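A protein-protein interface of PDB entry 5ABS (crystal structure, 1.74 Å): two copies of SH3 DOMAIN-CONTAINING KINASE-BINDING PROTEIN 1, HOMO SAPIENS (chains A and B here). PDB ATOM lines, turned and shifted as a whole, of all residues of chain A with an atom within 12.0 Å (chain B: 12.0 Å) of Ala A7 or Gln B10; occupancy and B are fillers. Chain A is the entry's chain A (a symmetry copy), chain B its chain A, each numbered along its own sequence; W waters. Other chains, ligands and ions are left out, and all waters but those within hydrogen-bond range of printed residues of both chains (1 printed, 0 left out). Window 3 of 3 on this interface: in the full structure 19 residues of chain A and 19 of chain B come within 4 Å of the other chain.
Ala A7 touches Gln B10, but with the chains exchanged Gln A10 does not touch Ala B7 (12.7 Å). Ser B9 touches its own counterpart, Ser A9. Ala A12 touches Val B13, but with the chains exchanged Val A13 does not touch Ala B12 (7.6 Å). Leu A16 touches Val B13, but with the chains exchanged Val A13 does not touch Leu B16 (6.7 Å).
Met A3 touches none of the printed residues of chain B. Pro A5 touches one residue of chain B. Ala A7 touches one residue of chain B. No residue of chain B comes within 4 Å of Ser A8. Ser A9 touches just one residue of chain B: Ser B9 (3.9 Å). No residue of chain B comes within 4 Å of Ala A11. Printed residues of chain B within 4 Å of Ala A12: Val B13 (3.6 Å) and Arg B17 (3.7 Å). Glu A14 touches none of the printed residues of chain B. Of the printed residues of chain B, Leu A16 touches Val B13, Leu B16 and Arg B17. Ser B9 touches just one residue of chain A: Ser A9. Of the printed residues of chain A, Gln B10 touches Ala A7. Val B13 touches two residues of chain A. No residue of chain A comes within 4 Å of Glu B14. Printed residues of chain A within 4 Å of Arg B17: Pro A5 (3.9 Å), Ala A6 (3.9 Å), Ala A12 (3.7 Å) and Leu A16 (3.98 Å). The nearest printed residue of chain A that does not touch Leu B16 is Gln A19 (6.3 Å).
The backbone NH (N) of Ala A6 is in hydrogen-bond range of the side-chain carboxylate (OE1) of Glu A15, at 3.1 Å.
Water W1 bridges O of Ala A12 and NH2 of Arg B17.
Printed residues of chain B that touch a printed residue of chain A: Ser B9, Gln B10, Val B13, Leu B16 and Arg B17. Along chain B the printed residues that touch a printed residue of chain A span positions 9 to 17. Among the printed residues, 9 pairs touch across the chains.
Among the printed residues, pairs that only touch across the chains: Ala A12 with Val B13, Ala A12 with Arg B17, Leu A16 with Val B13, Ala A6 with Arg B17, Pro A5 with Arg B17, Ala A7 with Gln B10, Ser A9 with Ser B9, Leu A16 with Leu B16 and Leu A16 with Arg B17.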
ATOM      1  N   MET A   3       2.717 -14.880 -22.692  1.00  0.00           N
ATOM      2  CA  MET A   3       1.502 -14.766 -23.547  1.00  0.00           C
ATOM      3  C   MET A   3       1.506 -13.485 -24.410  1.00  0.00           C
ATOM      4  O   MET A   3       1.829 -12.378 -23.930  1.00  0.00           O
ATOM      5  CB  MET A   3       0.198 -14.882 -22.723  1.00  0.00           C
ATOM      6  N   GLU A   4       1.152 -13.646 -25.700  1.00  0.00           N
ATOM      7  CA  GLU A   4       1.191 -12.549 -26.696  1.00  0.00           C
ATOM      8  C   GLU A   4       0.194 -11.480 -26.290  1.00  0.00           C
ATOM      9  O   GLU A   4      -0.899 -11.823 -25.861  1.00  0.00           O
ATOM     10  CB  GLU A   4       0.817 -13.042 -28.108  1.00  0.00           C
ATOM     11  CG  GLU A   4       1.804 -14.030 -28.718  1.00  0.00           C
ATOM     12  CD  GLU A   4       3.212 -13.427 -28.665  1.00  0.00           C
ATOM     13  OE1 GLU A   4       3.406 -12.360 -29.322  1.00  0.00           O
ATOM     14  OE2 GLU A   4       4.044 -13.954 -27.906  1.00  0.00           O
ATOM     15  N   PRO A   5       0.542 -10.196 -26.474  1.00  0.00           N
ATOM     16  CA  PRO A   5      -0.430  -9.113 -26.237  1.00  0.00           C
ATOM     17  C   PRO A   5      -1.650  -9.223 -27.126  1.00  0.00           C
ATOM     18  O   PRO A   5      -1.545  -9.720 -28.242  1.00  0.00           O
ATOM     19  CB  PRO A   5       0.340  -7.845 -26.610  1.00  0.00           C
ATOM     20  CG  PRO A   5       1.774  -8.236 -26.568  1.00  0.00           C
ATOM     21  CD  PRO A   5       1.815  -9.672 -26.991  1.00  0.00           C
ATOM     22  N   ALA A   6      -2.799  -8.760 -26.641  1.00  0.00           N
ATOM     23  CA  ALA A   6      -4.011  -8.714 -27.477  1.00  0.00           C
ATOM     24  C   ALA A   6      -3.785  -7.742 -28.606  1.00  0.00           C
ATOM     25  O   ALA A   6      -3.101  -6.722 -28.410  1.00  0.00           O
ATOM     26  CB  ALA A   6      -5.185  -8.250 -26.649  1.00  0.00           C
ATOM     27  N   ALA A   7      -4.347  -8.045 -29.773  1.00  0.00           N
ATOM     28  CA  ALA A   7      -4.293  -7.128 -30.936  1.00  0.00           C
ATOM     29  C   ALA A   7      -5.490  -6.154 -31.037  1.00  0.00           C
ATOM     30  O   ALA A   7      -5.297  -4.973 -31.363  1.00  0.00           O
ATOM     31  CB  ALA A   7      -4.169  -7.946 -32.219  1.00  0.00           C
ATOM     32  N   SER A   8      -6.702  -6.692 -30.841  1.00  0.00           N
ATOM     33  CA  SER A   8      -7.970  -5.955 -30.613  1.00  0.00           C
ATOM     34  C   SER A   8      -7.755  -4.780 -29.627  1.00  0.00           C
ATOM     35  O   SER A   8      -7.187  -4.983 -28.551  1.00  0.00           O
ATOM     36  CB  SER A   8      -8.990  -6.967 -30.023  1.00  0.00           C
ATOM     37  OG  SER A   8     -10.089  -6.316 -29.340  1.00  0.00           O
ATOM     38  N   SER A   9      -8.152  -3.560 -29.967  1.00  0.00           N
ATOM     39  CA  SER A   9      -7.936  -2.434 -29.054  1.00  0.00           C
ATOM     40  C   SER A   9      -8.650  -2.584 -27.693  1.00  0.00           C
ATOM     41  O   SER A   9      -8.040  -2.253 -26.687  1.00  0.00           O
ATOM     42  CB  SER A   9      -8.269  -1.079 -29.676  1.00  0.00           C
ATOM     43  OG  SER A   9      -7.095  -0.544 -30.260  1.00  0.00           O
ATOM     44  N   GLN A  10      -9.893  -3.072 -27.680  1.00  0.00           N
ATOM     45  CA  GLN A  10     -10.622  -3.226 -26.433  1.00  0.00           C
ATOM     46  C   GLN A  10      -9.989  -4.268 -25.558  1.00  0.00           C
ATOM     47  O   GLN A  10      -9.938  -4.099 -24.347  1.00  0.00           O
ATOM     48  CB  GLN A  10     -12.099  -3.597 -26.612  1.00  0.00           C
ATOM     49  CG  GLN A  10     -13.076  -2.456 -26.330  1.00  0.00           C
ATOM     50  CD  GLN A  10     -14.471  -2.996 -26.018  1.00  0.00           C
ATOM     51  OE1 GLN A  10     -15.119  -2.563 -25.054  1.00  0.00           O
ATOM     52  NE2 GLN A  10     -14.932  -3.973 -26.826  1.00  0.00           N
ATOM     53  N   ALA A  11      -9.524  -5.355 -26.155  1.00  0.00           N
ATOM     54  CA  ALA A  11      -8.855  -6.360 -25.379  1.00  0.00           C
ATOM     55  C   ALA A  11      -7.528  -5.801 -24.805  1.00  0.00           C
ATOM     56  O   ALA A  11      -7.175  -6.060 -23.638  1.00  0.00           O
ATOM     57  CB  ALA A  11      -8.620  -7.585 -26.241  1.00  0.00           C
ATOM     58  N   ALA A  12      -6.811  -5.003 -25.612  1.00  0.00           N
ATOM     59  CA  ALA A  12      -5.569  -4.442 -25.178  1.00  0.00           C
ATOM     60  C   ALA A  12      -5.734  -3.471 -24.007  1.00  0.00           C
ATOM     61  O   ALA A  12      -4.947  -3.478 -23.078  1.00  0.00           O
ATOM     62  CB  ALA A  12      -4.835  -3.817 -26.344  1.00  0.00           C
ATOM     63  N   VAL A  13      -6.781  -2.648 -24.071  1.00  0.00           N
ATOM     64  CA  VAL A  13      -7.158  -1.736 -22.979  1.00  0.00           C
ATOM     65  C   VAL A  13      -7.443  -2.518 -21.684  1.00  0.00           C
ATOM     66  O   VAL A  13      -6.975  -2.110 -20.611  1.00  0.00           O
ATOM     67  CB  VAL A  13      -8.357  -0.841 -23.398  1.00  0.00           C
ATOM     68  CG1 VAL A  13      -9.125  -0.226 -22.198  1.00  0.00           C
ATOM     69  CG2 VAL A  13      -7.829   0.238 -24.327  1.00  0.00           C
ATOM     70  N   GLU A  14      -8.181  -3.609 -21.794  1.00  0.00           N
ATOM     71  CA  GLU A  14      -8.516  -4.422 -20.648  1.00  0.00           C
ATOM     72  C   GLU A  14      -7.322  -5.115 -20.021  1.00  0.00           C
ATOM     73  O   GLU A  14      -7.221  -5.153 -18.803  1.00  0.00           O
ATOM     74  CB  GLU A  14      -9.650  -5.401 -20.959  1.00  0.00           C
ATOM     75  CG  GLU A  14     -10.934  -4.612 -21.056  1.00  0.00           C
ATOM     76  CD  GLU A  14     -12.076  -5.343 -21.693  1.00  0.00           C
ATOM     77  OE1 GLU A  14     -12.038  -6.610 -21.717  1.00  0.00           O
ATOM     78  OE2 GLU A  14     -13.021  -4.620 -22.162  1.00  0.00           O
ATOM     79  N   GLU A  15      -6.387  -5.612 -20.823  1.00  0.00           N
ATOM     80  CA  GLU A  15      -5.098  -6.058 -20.310  1.00  0.00           C
ATOM     81  C   GLU A  15      -4.302  -4.985 -19.569  1.00  0.00           C
ATOM     82  O   GLU A  15      -3.715  -5.254 -18.538  1.00  0.00           O
ATOM     83  CB  GLU A  15      -4.221  -6.659 -21.425  1.00  0.00           C
ATOM     84  CG  GLU A  15      -4.702  -8.002 -21.941  1.00  0.00           C
ATOM     85  CD  GLU A  15      -3.699  -8.746 -22.877  1.00  0.00           C
ATOM     86  OE1 GLU A  15      -2.813  -8.121 -23.559  1.00  0.00           O
ATOM     87  OE2 GLU A  15      -3.811 -10.002 -22.925  1.00  0.00           O
ATOM     88  N   LEU A  16      -4.282  -3.760 -20.084  1.00  0.00           N
ATOM     89  CA  LEU A  16      -3.568  -2.688 -19.454  1.00  0.00           C
ATOM     90  C   LEU A  16      -4.251  -2.281 -18.124  1.00  0.00           C
ATOM     91  O   LEU A  16      -3.572  -2.039 -17.126  1.00  0.00           O
ATOM     92  CB  LEU A  16      -3.416  -1.460 -20.364  1.00  0.00           C
ATOM     93  CG  LEU A  16      -2.309  -1.609 -21.431  1.00  0.00           C
ATOM     94  CD1 LEU A  16      -2.472  -0.536 -22.482  1.00  0.00           C
ATOM     95  CD2 LEU A  16      -0.916  -1.588 -20.824  1.00  0.00           C
ATOM     96  N   GLN A  19      -2.995  -4.823 -15.628  1.00  0.00           N
ATOM     97  CA  GLN A  19      -1.649  -4.521 -15.222  1.00  0.00           C
ATOM     98  C   GLN A  19      -1.543  -3.303 -14.287  1.00  0.00           C
ATOM     99  O   GLN A  19      -0.727  -3.263 -13.382  1.00  0.00           O
ATOM    100  CB  GLN A  19      -0.773  -4.285 -16.453  1.00  0.00           C
ATOM    101  CG  GLN A  19      -0.437  -5.567 -17.223  1.00  0.00           C
ATOM    102  CD  GLN A  19       0.297  -5.290 -18.549  1.00  0.00           C
ATOM    103  OE1 GLN A  19       0.838  -4.220 -18.752  1.00  0.00           O
ATOM    104  NE2 GLN A  19       0.281  -6.242 -19.460  1.00  0.00           N
ATOM    105  N   GLU B   4       4.097  14.827 -28.101  1.00  0.00           N
ATOM    106  CA  GLU B   4       2.618  14.758 -28.093  1.00  0.00           C
ATOM    107  C   GLU B   4       2.193  13.304 -28.013  1.00  0.00           C
ATOM    108  O   GLU B   4       2.800  12.473 -28.677  1.00  0.00           O
ATOM    109  CB  GLU B   4       2.007  15.366 -29.371  1.00  0.00           C
ATOM    110  CG  GLU B   4       2.232  16.865 -29.530  1.00  0.00           C
ATOM    111  CD  GLU B   4       1.758  17.580 -28.261  1.00  0.00           C
ATOM    112  OE1 GLU B   4       0.526  17.488 -27.974  1.00  0.00           O
ATOM    113  OE2 GLU B   4       2.616  18.114 -27.537  1.00  0.00           O
ATOM    114  N   PRO B   5       1.127  13.003 -27.255  1.00  0.00           N
ATOM    115  CA  PRO B   5       0.574  11.636 -27.246  1.00  0.00           C
ATOM    116  C   PRO B   5       0.102  11.192 -28.614  1.00  0.00           C
ATOM    117  O   PRO B   5      -0.327  12.023 -29.407  1.00  0.00           O
ATOM    118  CB  PRO B   5      -0.638  11.739 -26.316  1.00  0.00           C
ATOM    119  CG  PRO B   5      -0.410  12.976 -25.522  1.00  0.00           C
ATOM    120  CD  PRO B   5       0.319  13.915 -26.431  1.00  0.00           C
ATOM    121  N   ALA B   6       0.174   9.891 -28.889  1.00  0.00           N
ATOM    122  CA  ALA B   6      -0.372   9.352 -30.146  1.00  0.00           C
ATOM    123  C   ALA B   6      -1.867   9.543 -30.147  1.00  0.00           C
ATOM    124  O   ALA B   6      -2.498   9.451 -29.081  1.00  0.00           O
ATOM    125  CB  ALA B   6      -0.061   7.878 -30.247  1.00  0.00           C
ATOM    126  N   ALA B   7      -2.431   9.808 -31.322  1.00  0.00           N
ATOM    127  CA  ALA B   7      -3.900   9.916 -31.486  1.00  0.00           C
ATOM    128  C   ALA B   7      -4.599   8.590 -31.870  1.00  0.00           C
ATOM    129  O   ALA B   7      -5.681   8.291 -31.345  1.00  0.00           O
ATOM    130  CB  ALA B   7      -4.217  10.996 -32.516  1.00  0.00           C
ATOM    131  N   SER B   8      -4.009   7.875 -32.837  1.00  0.00           N
ATOM    132  CA  SER B   8      -4.304   6.467 -33.202  1.00  0.00           C
ATOM    133  C   SER B   8      -4.469   5.593 -31.934  1.00  0.00           C
ATOM    134  O   SER B   8      -3.607   5.628 -31.052  1.00  0.00           O
ATOM    135  CB  SER B   8      -3.112   5.953 -34.053  1.00  0.00           C
ATOM    136  OG  SER B   8      -3.038   4.507 -34.092  1.00  0.00           O
ATOM    137  N   SER B   9      -5.556   4.844 -31.794  1.00  0.00           N
ATOM    138  CA  SER B   9      -5.738   4.027 -30.590  1.00  0.00           C
ATOM    139  C   SER B   9      -4.641   2.959 -30.385  1.00  0.00           C
ATOM    140  O   SER B   9      -4.212   2.789 -29.253  1.00  0.00           O
ATOM    141  CB  SER B   9      -7.121   3.386 -30.497  1.00  0.00           C
ATOM    142  OG  SER B   9      -7.977   4.250 -29.772  1.00  0.00           O
ATOM    143  N   GLN B  10      -4.212   2.279 -31.451  1.00  0.00           N
ATOM    144  CA  GLN B  10      -3.192   1.254 -31.321  1.00  0.00           C
ATOM    145  C   GLN B  10      -1.873   1.846 -30.919  1.00  0.00           C
ATOM    146  O   GLN B  10      -1.154   1.252 -30.127  1.00  0.00           O
ATOM    147  CB  GLN B  10      -2.967   0.428 -32.594  1.00  0.00           C
ATOM    148  CG  GLN B  10      -3.531  -0.991 -32.535  1.00  0.00           C
ATOM    149  CD  GLN B  10      -2.848  -1.892 -33.563  1.00  0.00           C
ATOM    150  OE1 GLN B  10      -2.449  -3.023 -33.250  1.00  0.00           O
ATOM    151  NE2 GLN B  10      -2.687  -1.380 -34.800  1.00  0.00           N
ATOM    152  N   ALA B  11      -1.539   3.003 -31.470  1.00  0.00           N
ATOM    153  CA  ALA B  11      -0.317   3.648 -31.081  1.00  0.00           C
ATOM    154  C   ALA B  11      -0.392   4.090 -29.596  1.00  0.00           C
ATOM    155  O   ALA B  11       0.585   3.952 -28.836  1.00  0.00           O
ATOM    156  CB  ALA B  11      -0.056   4.824 -32.001  1.00  0.00           C
ATOM    157  N   ALA B  12      -1.567   4.585 -29.174  1.00  0.00           N
ATOM    158  CA  ALA B  12      -1.736   5.027 -27.823  1.00  0.00           C
ATOM    159  C   ALA B  12      -1.605   3.890 -26.808  1.00  0.00           C
ATOM    160  O   ALA B  12      -0.998   4.055 -25.766  1.00  0.00           O
ATOM    161  CB  ALA B  12      -3.038   5.784 -27.674  1.00  0.00           C
ATOM    162  N   VAL B  13      -2.179   2.734 -27.145  1.00  0.00           N
ATOM    163  CA  VAL B  13      -2.049   1.506 -26.343  1.00  0.00           C
ATOM    164  C   VAL B  13      -0.570   1.100 -26.196  1.00  0.00           C
ATOM    165  O   VAL B  13      -0.141   0.757 -25.085  1.00  0.00           O
ATOM    166  CB  VAL B  13      -2.912   0.362 -26.944  1.00  0.00           C
ATOM    167  CG1 VAL B  13      -2.472  -1.055 -26.491  1.00  0.00           C
ATOM    168  CG2 VAL B  13      -4.360   0.634 -26.580  1.00  0.00           C
ATOM    169  N   GLU B  14       0.176   1.151 -27.287  1.00  0.00           N
ATOM    170  CA  GLU B  14       1.574   0.790 -27.271  1.00  0.00           C
ATOM    171  C   GLU B  14       2.438   1.734 -26.459  1.00  0.00           C
ATOM    172  O   GLU B  14       3.309   1.277 -25.731  1.00  0.00           O
ATOM    173  CB  GLU B  14       2.121   0.583 -28.684  1.00  0.00           C
ATOM    174  CG  GLU B  14       1.564  -0.716 -29.215  1.00  0.00           C
ATOM    175  CD  GLU B  14       1.707  -0.906 -30.695  1.00  0.00           C
ATOM    176  OE1 GLU B  14       2.594  -0.234 -31.301  1.00  0.00           O
ATOM    177  OE2 GLU B  14       0.917  -1.754 -31.236  1.00  0.00           O
ATOM    178  N   GLU B  15       2.181   3.037 -26.521  1.00  0.00           N
ATOM    179  CA  GLU B  15       2.784   3.979 -25.587  1.00  0.00           C
ATOM    180  C   GLU B  15       2.487   3.696 -24.115  1.00  0.00           C
ATOM    181  O   GLU B  15       3.365   3.799 -23.278  1.00  0.00           O
ATOM    182  CB  GLU B  15       2.387   5.433 -25.913  1.00  0.00           C
ATOM    183  CG  GLU B  15       3.016   5.981 -27.180  1.00  0.00           C
ATOM    184  CD  GLU B  15       2.838   7.517 -27.391  1.00  0.00           C
ATOM    185  OE1 GLU B  15       1.866   8.168 -26.870  1.00  0.00           O
ATOM    186  OE2 GLU B  15       3.709   8.084 -28.107  1.00  0.00           O
ATOM    187  N   LEU B  16       1.252   3.332 -23.789  1.00  0.00           N
ATOM    188  CA  LEU B  16       0.884   3.040 -22.435  1.00  0.00           C
ATOM    189  C   LEU B  16       1.559   1.731 -21.955  1.00  0.00           C
ATOM    190  O   LEU B  16       2.042   1.660 -20.825  1.00  0.00           O
ATOM    191  CB  LEU B  16      -0.636   2.949 -22.240  1.00  0.00           C
ATOM    192  CG  LEU B  16      -1.338   4.324 -22.163  1.00  0.00           C
ATOM    193  CD1 LEU B  16      -2.828   4.143 -22.333  1.00  0.00           C
ATOM    194  CD2 LEU B  16      -1.008   5.068 -20.880  1.00  0.00           C
ATOM    195  N   ARG B  17       1.680   0.791 -22.849  1.00  0.00           N
ATOM    196  CA  ARG B  17       2.463  -0.428 -22.578  1.00  0.00           C
ATOM    197  C   ARG B  17       3.929  -0.084 -22.198  1.00  0.00           C
ATOM    198  O   ARG B  17       4.492  -0.605 -21.246  1.00  0.00           O
ATOM    199  CB  ARG B  17       2.468  -1.305 -23.835  1.00  0.00           C
ATOM    200  CG  ARG B  17       2.539  -2.755 -23.565  1.00  0.00           C
ATOM    201  CD  ARG B  17       2.150  -3.512 -24.812  1.00  0.00           C
ATOM    202  NE  ARG B  17       0.727  -3.747 -24.961  1.00  0.00           N
ATOM    203  CZ  ARG B  17       0.096  -3.959 -26.116  1.00  0.00           C
ATOM    204  NH1 ARG B  17       0.724  -3.820 -27.308  1.00  0.00           N
ATOM    205  NH2 ARG B  17      -1.193  -4.258 -26.097  1.00  0.00           N
ATOM    206  N   THR B  18       4.530   0.780 -22.971  1.00  0.00           N
ATOM    207  CA  THR B  18       5.862   1.257 -22.690  1.00  0.00           C
ATOM    208  C   THR B  18       5.984   1.923 -21.315  1.00  0.00           C
ATOM    209  O   THR B  18       6.938   1.680 -20.615  1.00  0.00           O
ATOM    210  CB  THR B  18       6.364   2.166 -23.822  1.00  0.00           C
ATOM    211  OG1 THR B  18       6.383   1.409 -25.039  1.00  0.00           O
ATOM    212  CG2 THR B  18       7.779   2.672 -23.530  1.00  0.00           C
ATOM    213  N   GLN B  19       5.044   2.799 -20.965  1.00  0.00           N
ATOM    214  CA  GLN B  19       5.034   3.459 -19.687  1.00  0.00           C
ATOM    215  C   GLN B  19       4.807   2.506 -18.500  1.00  0.00           C
ATOM    216  O   GLN B  19       5.363   2.679 -17.428  1.00  0.00           O
ATOM    217  CB  GLN B  19       3.958   4.544 -19.670  1.00  0.00           C
ATOM    218  CG  GLN B  19       4.318   5.782 -20.498  1.00  0.00           C
ATOM    219  CD  GLN B  19       3.154   6.785 -20.608  1.00  0.00           C
ATOM    220  OE1 GLN B  19       2.217   6.742 -19.835  1.00  0.00           O
ATOM    221  NE2 GLN B  19       3.201   7.661 -21.591  1.00  0.00           N
ATOM    222  N   ARG B  21       5.900  -0.732 -18.636  1.00  0.00           N
ATOM    223  CA  ARG B  21       7.282  -1.296 -18.518  1.00  0.00           C
ATOM    224  C   ARG B  21       8.240  -0.335 -17.784  1.00  0.00           C
ATOM    225  O   ARG B  21       9.005  -0.780 -16.932  1.00  0.00           O
ATOM    226  CB  ARG B  21       7.916  -1.717 -19.859  1.00  0.00           C
ATOM    227  CG  ARG B  21       7.332  -2.928 -20.605  1.00  0.00           C
ATOM    228  CD  ARG B  21       8.267  -3.447 -21.747  1.00  0.00           C
ATOM    229  NE  ARG B  21       8.698  -2.422 -22.733  1.00  0.00           N
ATOM    230  CZ  ARG B  21       7.953  -1.928 -23.737  1.00  0.00           C
ATOM    231  NH1 ARG B  21       6.700  -2.349 -23.968  1.00  0.00           N
ATOM    232  NH2 ARG B  21       8.469  -0.971 -24.529  1.00  0.00           N
HETATM  233  O   HOH W   1      -2.505  -4.518 -23.630  1.00  0.00           O
